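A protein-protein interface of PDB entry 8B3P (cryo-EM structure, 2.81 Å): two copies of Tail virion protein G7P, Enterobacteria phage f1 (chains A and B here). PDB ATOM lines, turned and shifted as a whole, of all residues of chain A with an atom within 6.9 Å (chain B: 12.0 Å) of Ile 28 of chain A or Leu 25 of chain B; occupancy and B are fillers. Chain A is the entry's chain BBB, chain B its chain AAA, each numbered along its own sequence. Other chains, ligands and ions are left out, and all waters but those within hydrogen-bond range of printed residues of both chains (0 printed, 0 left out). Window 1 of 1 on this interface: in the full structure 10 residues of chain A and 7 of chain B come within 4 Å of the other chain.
O of Ile 28 of chain A sits close to OE1 of Gln 32 of chain B, at 2.9 Å. The backbone carbonyl oxygen of Gly 31 of chain A lies close to the side-chain amide nitrogen of Gln 32 of chain B (3.0 Å). The side-chain amide nitrogen of Gln 32 of chain B lies close to the backbone NH of Gln 32 of chain A.
SG of Cys 22 of chain B sits at hydrogen-bond distance from O of Ser 18 of chain B, 3.3 Å away.
Among the printed residues, pairs that only touch across the chains: Leu 21 of chain A with Cys 22 of chain B, Leu 21 of chain A with Leu 25 of chain B, Ala 24 of chain A with Leu 25 of chain B and Ile 28 of chain A with Leu 25 of chain B.
Leu 21 of chain A touches two residues of chain B. Ala 24 of chain A touches one residue of chain B. No residue of chain B comes within 4 Å of Leu 25 of chain A. Gly 26 of chain A touches none of the printed residues of chain B. No residue of chain B comes within 4 Å of Ile 27 of chain A. Ile 28 of chain A touches just these residues of chain B: Leu 25 and Gln 32. No residue of chain B comes within 4 Å of Gly 30 of chain A. Of chain B, only Gln 32 (3.2 Å) comes within 4 Å of Gln 32 of chain A. Of the printed residues of chain A, Cys 22 of chain B touches Leu 21. Leu 25 of chain B touches three residues of chain A. Of the printed residues of chain A, Gln 32 of chain B touches Ile 28 (2.9 Å), Gly 31 (3.0 Å) and Gln 32 (3.2 Å). The nearest residue of chain A that does not touch Leu 25 of chain B is Leu 25 of chain A (4.1 Å). The nearest printed residue of chain A that does not touch Gln 32 of chain B is Ile 27 of chain A (4.5 Å).
Of the 13 printed residues of chain A, 5 touch a printed residue of chain B. Of the 18 printed residues of chain B, 3 touch a printed residue of chain A. Printed residues of chain B that touch a printed residue of chain A: Cys 22, Leu 25 and Gln 32. Hydrophobic or aromatic side chains of chain B that line the printed part of chain A: Leu 25. Along chain B the printed residues that touch a printed residue of chain A span positions 22 to 32. Among the printed residues, 7 pairs touch across the chains. Among the printed residues, no Asp or Glu carboxylate lies within 4 Å of a Lys or Arg side-chain nitrogen of the other chain.
Leu 21 of chain A touches Cys 22 of chain B, but with the chains exchanged Cys 22 of chain A does not touch Leu 21 of chain B (9.5 Å). Ala 24 of chain A touches Leu 25 of chain B, but with the chains exchanged Leu 25 of chain A does not touch Ala 24 of chain B (8.9 Å). Ile 28 of chain A touches Gln 32 of chain B, but with the chains exchanged Gln 32 of chain A does not touch Ile 28 of chain B (8.6 Å). Gln 32 of chain A touches its own counterpart, Gln 32 of chain B.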
ATOM      1  N   VAL A  20      -1.209  -5.659   8.845  1.00  0.00           N
ATOM      2  CA  VAL A  20      -2.529  -5.093   8.584  1.00  0.00           C
ATOM      3  C   VAL A  20      -2.410  -3.676   8.016  1.00  0.00           C
ATOM      4  O   VAL A  20      -3.174  -3.325   7.118  1.00  0.00           O
ATOM      5  CB  VAL A  20      -3.458  -5.158   9.817  1.00  0.00           C
ATOM      6  CG1 VAL A  20      -4.846  -4.593   9.536  1.00  0.00           C
ATOM      7  CG2 VAL A  20      -3.573  -6.574  10.366  1.00  0.00           C
ATOM      8  N   LEU A  21      -1.452  -2.878   8.519  1.00  0.00           N
ATOM      9  CA  LEU A  21      -1.339  -1.486   8.097  1.00  0.00           C
ATOM     10  C   LEU A  21      -0.843  -1.381   6.653  1.00  0.00           C
ATOM     11  O   LEU A  21      -1.185  -0.420   5.963  1.00  0.00           O
ATOM     12  CB  LEU A  21      -0.440  -0.681   9.045  1.00  0.00           C
ATOM     13  CG  LEU A  21      -1.063  -0.169  10.347  1.00  0.00           C
ATOM     14  CD1 LEU A  21      -0.074   0.705  11.102  1.00  0.00           C
ATOM     15  CD2 LEU A  21      -2.357   0.595  10.111  1.00  0.00           C
ATOM     16  N   CYS A  22      -0.058  -2.368   6.197  1.00  0.00           N
ATOM     17  CA  CYS A  22       0.474  -2.344   4.841  1.00  0.00           C
ATOM     18  C   CYS A  22      -0.549  -2.877   3.840  1.00  0.00           C
ATOM     19  O   CYS A  22      -0.444  -2.592   2.649  1.00  0.00           O
ATOM     20  CB  CYS A  22       1.785  -3.111   4.736  1.00  0.00           C
ATOM     21  SG  CYS A  22       3.066  -2.452   5.831  1.00  0.00           S
ATOM     22  N   PHE A  23      -1.519  -3.658   4.336  1.00  0.00           N
ATOM     23  CA  PHE A  23      -2.638  -4.135   3.537  1.00  0.00           C
ATOM     24  C   PHE A  23      -3.570  -2.970   3.201  1.00  0.00           C
ATOM     25  O   PHE A  23      -3.989  -2.829   2.052  1.00  0.00           O
ATOM     26  CB  PHE A  23      -3.357  -5.294   4.237  1.00  0.00           C
ATOM     27  CG  PHE A  23      -4.501  -5.873   3.443  1.00  0.00           C
ATOM     28  CD1 PHE A  23      -4.268  -6.792   2.426  1.00  0.00           C
ATOM     29  CD2 PHE A  23      -5.811  -5.476   3.688  1.00  0.00           C
ATOM     30  CE1 PHE A  23      -5.321  -7.307   1.679  1.00  0.00           C
ATOM     31  CE2 PHE A  23      -6.864  -5.987   2.938  1.00  0.00           C
ATOM     32  CZ  PHE A  23      -6.615  -6.905   1.939  1.00  0.00           C
ATOM     33  N   ALA A  24      -3.869  -2.140   4.212  1.00  0.00           N
ATOM     34  CA  ALA A  24      -4.816  -1.038   4.113  1.00  0.00           C
ATOM     35  C   ALA A  24      -4.303   0.036   3.152  1.00  0.00           C
ATOM     36  O   ALA A  24      -5.073   0.580   2.358  1.00  0.00           O
ATOM     37  CB  ALA A  24      -5.097  -0.482   5.487  1.00  0.00           C
ATOM     38  N   LEU A  25      -2.994   0.318   3.220  1.00  0.00           N
ATOM     39  CA  LEU A  25      -2.349   1.264   2.321  1.00  0.00           C
ATOM     40  C   LEU A  25      -2.320   0.720   0.892  1.00  0.00           C
ATOM     41  O   LEU A  25      -2.426   1.491  -0.057  1.00  0.00           O
ATOM     42  CB  LEU A  25      -0.938   1.571   2.830  1.00  0.00           C
ATOM     43  CG  LEU A  25      -0.861   2.348   4.143  1.00  0.00           C
ATOM     44  CD1 LEU A  25       0.566   2.373   4.655  1.00  0.00           C
ATOM     45  CD2 LEU A  25      -1.387   3.768   3.982  1.00  0.00           C
ATOM     46  N   GLY A  26      -2.159  -0.604   0.754  1.00  0.00           N
ATOM     47  CA  GLY A  26      -2.270  -1.283  -0.528  1.00  0.00           C
ATOM     48  C   GLY A  26      -3.641  -1.082  -1.169  1.00  0.00           C
ATOM     49  O   GLY A  26      -3.720  -0.770  -2.357  1.00  0.00           O
ATOM     50  N   ILE A  27      -4.700  -1.260  -0.360  1.00  0.00           N
ATOM     51  CA  ILE A  27      -6.084  -1.144  -0.805  1.00  0.00           C
ATOM     52  C   ILE A  27      -6.342   0.276  -1.308  1.00  0.00           C
ATOM     53  O   ILE A  27      -7.019   0.446  -2.320  1.00  0.00           O
ATOM     54  CB  ILE A  27      -7.093  -1.563   0.293  1.00  0.00           C
ATOM     55  CG1 ILE A  27      -7.044  -3.062   0.625  1.00  0.00           C
ATOM     56  CG2 ILE A  27      -8.511  -1.090  -0.027  1.00  0.00           C
ATOM     57  CD1 ILE A  27      -7.911  -3.964  -0.241  1.00  0.00           C
ATOM     58  N   ILE A  28      -5.797   1.274  -0.601  1.00  0.00           N
ATOM     59  CA  ILE A  28      -6.045   2.671  -0.923  1.00  0.00           C
ATOM     60  C   ILE A  28      -5.354   3.011  -2.243  1.00  0.00           C
ATOM     61  O   ILE A  28      -5.911   3.741  -3.060  1.00  0.00           O
ATOM     62  CB  ILE A  28      -5.621   3.592   0.242  1.00  0.00           C
ATOM     63  CG1 ILE A  28      -6.547   3.412   1.451  1.00  0.00           C
ATOM     64  CG2 ILE A  28      -5.526   5.052  -0.192  1.00  0.00           C
ATOM     65  CD1 ILE A  28      -6.028   4.022   2.741  1.00  0.00           C
ATOM     66  N   ALA A  29      -4.163   2.431  -2.445  1.00  0.00           N
ATOM     67  CA  ALA A  29      -3.329   2.663  -3.614  1.00  0.00           C
ATOM     68  C   ALA A  29      -4.026   2.134  -4.864  1.00  0.00           C
ATOM     69  O   ALA A  29      -3.855   2.686  -5.953  1.00  0.00           O
ATOM     70  CB  ALA A  29      -1.991   1.993  -3.417  1.00  0.00           C
ATOM     71  N   GLY A  30      -4.827   1.077  -4.658  1.00  0.00           N
ATOM     72  CA  GLY A  30      -5.440   0.276  -5.706  1.00  0.00           C
ATOM     73  C   GLY A  30      -6.677   0.930  -6.314  1.00  0.00           C
ATOM     74  O   GLY A  30      -6.961   0.726  -7.495  1.00  0.00           O
ATOM     75  N   GLY A  31      -7.391   1.716  -5.494  1.00  0.00           N
ATOM     76  CA  GLY A  31      -8.621   2.379  -5.890  1.00  0.00           C
ATOM     77  C   GLY A  31      -8.383   3.773  -6.465  1.00  0.00           C
ATOM     78  O   GLY A  31      -9.347   4.482  -6.750  1.00  0.00           O
ATOM     79  N   GLN A  32      -7.105   4.162  -6.589  1.00  0.00           N
ATOM     80  CA  GLN A  32      -6.713   5.390  -7.262  1.00  0.00           C
ATOM     81  C   GLN A  32      -6.874   5.195  -8.767  1.00  0.00           C
ATOM     82  O   GLN A  32      -6.250   4.307  -9.346  1.00  0.00           O
ATOM     83  CB  GLN A  32      -5.293   5.794  -6.863  1.00  0.00           C
ATOM     84  CG  GLN A  32      -5.250   6.582  -5.555  1.00  0.00           C
ATOM     85  CD  GLN A  32      -3.944   7.266  -5.228  1.00  0.00           C
ATOM     86  OE1 GLN A  32      -3.194   6.858  -4.338  1.00  0.00           O
ATOM     87  NE2 GLN A  32      -3.677   8.359  -5.920  1.00  0.00           N
ATOM     88  N   GLN B  16      -4.583   0.041  21.579  1.00  0.00           N
ATOM     89  CA  GLN B  16      -5.578   1.101  21.496  1.00  0.00           C
ATOM     90  C   GLN B  16      -5.345   1.982  20.266  1.00  0.00           C
ATOM     91  O   GLN B  16      -6.282   2.215  19.504  1.00  0.00           O
ATOM     92  CB  GLN B  16      -5.680   1.881  22.809  1.00  0.00           C
ATOM     93  CG  GLN B  16      -6.703   1.298  23.774  1.00  0.00           C
ATOM     94  CD  GLN B  16      -6.303   1.443  25.222  1.00  0.00           C
ATOM     95  OE1 GLN B  16      -6.171   2.549  25.745  1.00  0.00           O
ATOM     96  NE2 GLN B  16      -6.121   0.315  25.891  1.00  0.00           N
ATOM     97  N   ILE B  17      -4.093   2.415  20.050  1.00  0.00           N
ATOM     98  CA  ILE B  17      -3.735   3.249  18.909  1.00  0.00           C
ATOM     99  C   ILE B  17      -3.992   2.492  17.600  1.00  0.00           C
ATOM    100  O   ILE B  17      -4.556   3.059  16.666  1.00  0.00           O
ATOM    101  CB  ILE B  17      -2.297   3.805  19.031  1.00  0.00           C
ATOM    102  CG1 ILE B  17      -2.121   4.640  20.306  1.00  0.00           C
ATOM    103  CG2 ILE B  17      -1.905   4.593  17.785  1.00  0.00           C
ATOM    104  CD1 ILE B  17      -0.677   4.964  20.670  1.00  0.00           C
ATOM    105  N   SER B  18      -3.624   1.202  17.558  1.00  0.00           N
ATOM    106  CA  SER B  18      -3.771   0.339  16.390  1.00  0.00           C
ATOM    107  C   SER B  18      -5.211   0.300  15.881  1.00  0.00           C
ATOM    108  O   SER B  18      -5.443   0.488  14.690  1.00  0.00           O
ATOM    109  CB  SER B  18      -3.256  -1.047  16.665  1.00  0.00           C
ATOM    110  OG  SER B  18      -1.841  -1.046  16.598  1.00  0.00           O
ATOM    111  N   VAL B  19      -6.159   0.061  16.795  1.00  0.00           N
ATOM    112  CA  VAL B  19      -7.572  -0.066  16.472  1.00  0.00           C
ATOM    113  C   VAL B  19      -8.066   1.206  15.774  1.00  0.00           C
ATOM    114  O   VAL B  19      -8.696   1.113  14.722  1.00  0.00           O
ATOM    115  CB  VAL B  19      -8.394  -0.473  17.714  1.00  0.00           C
ATOM    116  CG1 VAL B  19      -9.894  -0.458  17.473  1.00  0.00           C
ATOM    117  CG2 VAL B  19      -7.975  -1.845  18.227  1.00  0.00           C
ATOM    118  N   VAL B  20      -7.711   2.381  16.319  1.00  0.00           N
ATOM    119  CA  VAL B  20      -8.152   3.665  15.782  1.00  0.00           C
ATOM    120  C   VAL B  20      -7.520   3.924  14.411  1.00  0.00           C
ATOM    121  O   VAL B  20      -8.199   4.444  13.526  1.00  0.00           O
ATOM    122  CB  VAL B  20      -7.920   4.834  16.765  1.00  0.00           C
ATOM    123  CG1 VAL B  20      -8.408   6.169  16.214  1.00  0.00           C
ATOM    124  CG2 VAL B  20      -8.558   4.566  18.121  1.00  0.00           C
ATOM    125  N   LEU B  21      -6.240   3.553  14.230  1.00  0.00           N
ATOM    126  CA  LEU B  21      -5.540   3.854  12.986  1.00  0.00           C
ATOM    127  C   LEU B  21      -6.078   3.013  11.827  1.00  0.00           C
ATOM    128  O   LEU B  21      -6.038   3.464  10.682  1.00  0.00           O
ATOM    129  CB  LEU B  21      -4.023   3.678  13.135  1.00  0.00           C
ATOM    130  CG  LEU B  21      -3.237   4.823  13.780  1.00  0.00           C
ATOM    131  CD1 LEU B  21      -1.745   4.532  13.736  1.00  0.00           C
ATOM    132  CD2 LEU B  21      -3.524   6.165  13.125  1.00  0.00           C
ATOM    133  N   CYS B  22      -6.593   1.812  12.124  1.00  0.00           N
ATOM    134  CA  CYS B  22      -7.113   0.935  11.082  1.00  0.00           C
ATOM    135  C   CYS B  22      -8.548   1.308  10.718  1.00  0.00           C
ATOM    136  O   CYS B  22      -9.015   0.955   9.635  1.00  0.00           O
ATOM    137  CB  CYS B  22      -7.021  -0.530  11.483  1.00  0.00           C
ATOM    138  SG  CYS B  22      -5.321  -1.050  11.827  1.00  0.00           S
ATOM    139  N   PHE B  23      -9.235   2.009  11.631  1.00  0.00           N
ATOM    140  CA  PHE B  23     -10.562   2.550  11.382  1.00  0.00           C
ATOM    141  C   PHE B  23     -10.473   3.701  10.378  1.00  0.00           C
ATOM    142  O   PHE B  23     -11.266   3.761   9.438  1.00  0.00           O
ATOM    143  CB  PHE B  23     -11.247   2.951  12.693  1.00  0.00           C
ATOM    144  CG  PHE B  23     -12.649   3.477  12.515  1.00  0.00           C
ATOM    145  CD1 PHE B  23     -13.723   2.607  12.362  1.00  0.00           C
ATOM    146  CD2 PHE B  23     -12.894   4.846  12.468  1.00  0.00           C
ATOM    147  CE1 PHE B  23     -15.011   3.095  12.176  1.00  0.00           C
ATOM    148  CE2 PHE B  23     -14.181   5.333  12.277  1.00  0.00           C
ATOM    149  CZ  PHE B  23     -15.238   4.456  12.137  1.00  0.00           C
ATOM    150  N   ALA B  24      -9.492   4.593  10.587  1.00  0.00           N
ATOM    151  CA  ALA B  24      -9.313   5.809   9.804  1.00  0.00           C
ATOM    152  C   ALA B  24      -8.937   5.473   8.359  1.00  0.00           C
ATOM    153  O   ALA B  24      -9.435   6.104   7.425  1.00  0.00           O
ATOM    154  CB  ALA B  24      -8.286   6.694  10.465  1.00  0.00           C
ATOM    155  N   LEU B  25      -8.072   4.464   8.189  1.00  0.00           N
ATOM    156  CA  LEU B  25      -7.677   3.984   6.873  1.00  0.00           C
ATOM    157  C   LEU B  25      -8.852   3.305   6.169  1.00  0.00           C
ATOM    158  O   LEU B  25      -8.969   3.397   4.950  1.00  0.00           O
ATOM    159  CB  LEU B  25      -6.485   3.032   7.013  1.00  0.00           C
ATOM    160  CG  LEU B  25      -5.176   3.670   7.474  1.00  0.00           C
ATOM    161  CD1 LEU B  25      -4.157   2.597   7.802  1.00  0.00           C
ATOM    162  CD2 LEU B  25      -4.617   4.622   6.427  1.00  0.00           C
ATOM    163  N   GLY B  26      -9.702   2.615   6.943  1.00  0.00           N
ATOM    164  CA  GLY B  26     -10.947   2.053   6.442  1.00  0.00           C
ATOM    165  C   GLY B  26     -11.871   3.122   5.865  1.00  0.00           C
ATOM    166  O   GLY B  26     -12.409   2.939   4.775  1.00  0.00           O
ATOM    167  N   ILE B  27     -12.031   4.227   6.613  1.00  0.00           N
ATOM    168  CA  ILE B  27     -12.902   5.336   6.240  1.00  0.00           C
ATOM    169  C   ILE B  27     -12.416   5.946   4.926  1.00  0.00           C
ATOM    170  O   ILE B  27     -13.238   6.282   4.075  1.00  0.00           O
ATOM    171  CB  ILE B  27     -13.019   6.398   7.363  1.00  0.00           C
ATOM    172  CG1 ILE B  27     -13.758   5.888   8.609  1.00  0.00           C
ATOM    173  CG2 ILE B  27     -13.600   7.714   6.845  1.00  0.00           C
ATOM    174  CD1 ILE B  27     -15.273   6.026   8.586  1.00  0.00           C
ATOM    175  N   ILE B  28     -11.092   6.074   4.774  1.00  0.00           N
ATOM    176  CA  ILE B  28     -10.508   6.724   3.611  1.00  0.00           C
ATOM    177  C   ILE B  28     -10.726   5.842   2.382  1.00  0.00           C
ATOM    178  O   ILE B  28     -11.015   6.351   1.302  1.00  0.00           O
ATOM    179  CB  ILE B  28      -9.025   7.074   3.856  1.00  0.00           C
ATOM    180  CG1 ILE B  28      -8.887   8.188   4.899  1.00  0.00           C
ATOM    181  CG2 ILE B  28      -8.294   7.412   2.558  1.00  0.00           C
ATOM    182  CD1 ILE B  28      -7.481   8.373   5.443  1.00  0.00           C
ATOM    183  N   ALA B  29     -10.630   4.520   2.588  1.00  0.00           N
ATOM    184  CA  ALA B  29     -10.757   3.519   1.540  1.00  0.00           C
ATOM    185  C   ALA B  29     -12.175   3.531   0.979  1.00  0.00           C
ATOM    186  O   ALA B  29     -12.378   3.251  -0.204  1.00  0.00           O
ATOM    187  CB  ALA B  29     -10.410   2.161   2.100  1.00  0.00           C
ATOM    188  N   GLY B  30     -13.127   3.889   1.856  1.00  0.00           N
ATOM    189  CA  GLY B  30     -14.557   3.788   1.621  1.00  0.00           C
ATOM    190  C   GLY B  30     -15.107   4.923   0.762  1.00  0.00           C
ATOM    191  O   GLY B  30     -16.072   4.722   0.025  1.00  0.00           O
ATOM    192  N   GLY B  31     -14.473   6.101   0.867  1.00  0.00           N
ATOM    193  CA  GLY B  31     -14.889   7.296   0.155  1.00  0.00           C
ATOM    194  C   GLY B  31     -14.214   7.442  -1.207  1.00  0.00           C
ATOM    195  O   GLY B  31     -14.404   8.460  -1.870  1.00  0.00           O
ATOM    196  N   GLN B  32     -13.405   6.440  -1.585  1.00  0.00           N
ATOM    197  CA  GLN B  32     -12.819   6.357  -2.913  1.00  0.00           C
ATOM    198  C   GLN B  32     -13.906   5.944  -3.902  1.00  0.00           C
ATOM    199  O   GLN B  32     -14.506   4.882  -3.753  1.00  0.00           O
ATOM    200  CB  GLN B  32     -11.623   5.402  -2.919  1.00  0.00           C
ATOM    201  CG  GLN B  32     -10.328   6.071  -2.462  1.00  0.00           C
ATOM    202  CD  GLN B  32      -9.039   5.342  -2.762  1.00  0.00           C
ATOM    203  OE1 GLN B  32      -8.407   4.741  -1.890  1.00  0.00           O
ATOM    204  NE2 GLN B  32      -8.601   5.441  -4.004  1.00  0.00           N
ATOM    205  N   ARG B  33     -14.177   6.830  -4.873  1.00  0.00           N
ATOM    206  CA  ARG B  33     -15.126   6.581  -5.948  1.00  0.00           C
ATOM    207  C   ARG B  33     -14.484   5.636  -6.978  1.00  0.00           C
ATOM    208  O   ARG B  33     -14.386   6.029  -8.164  1.00  0.00           O
ATOM    209  CB  ARG B  33     -15.633   7.905  -6.541  1.00  0.00           C
ATOM    210  CG  ARG B  33     -16.980   8.375  -6.002  1.00  0.00           C
ATOM    211  CD  ARG B  33     -17.595   9.516  -6.800  1.00  0.00           C
ATOM    212  NE  ARG B  33     -17.774  10.759  -6.051  1.00  0.00           N
ATOM    213  CZ  ARG B  33     -18.936  11.390  -5.862  1.00  0.00           C
ATOM    214  NH1 ARG B  33     -20.056  10.910  -6.379  1.00  0.00           N
ATOM    215  NH2 ARG B  33     -18.977  12.510  -5.161  1.00  0.00           N
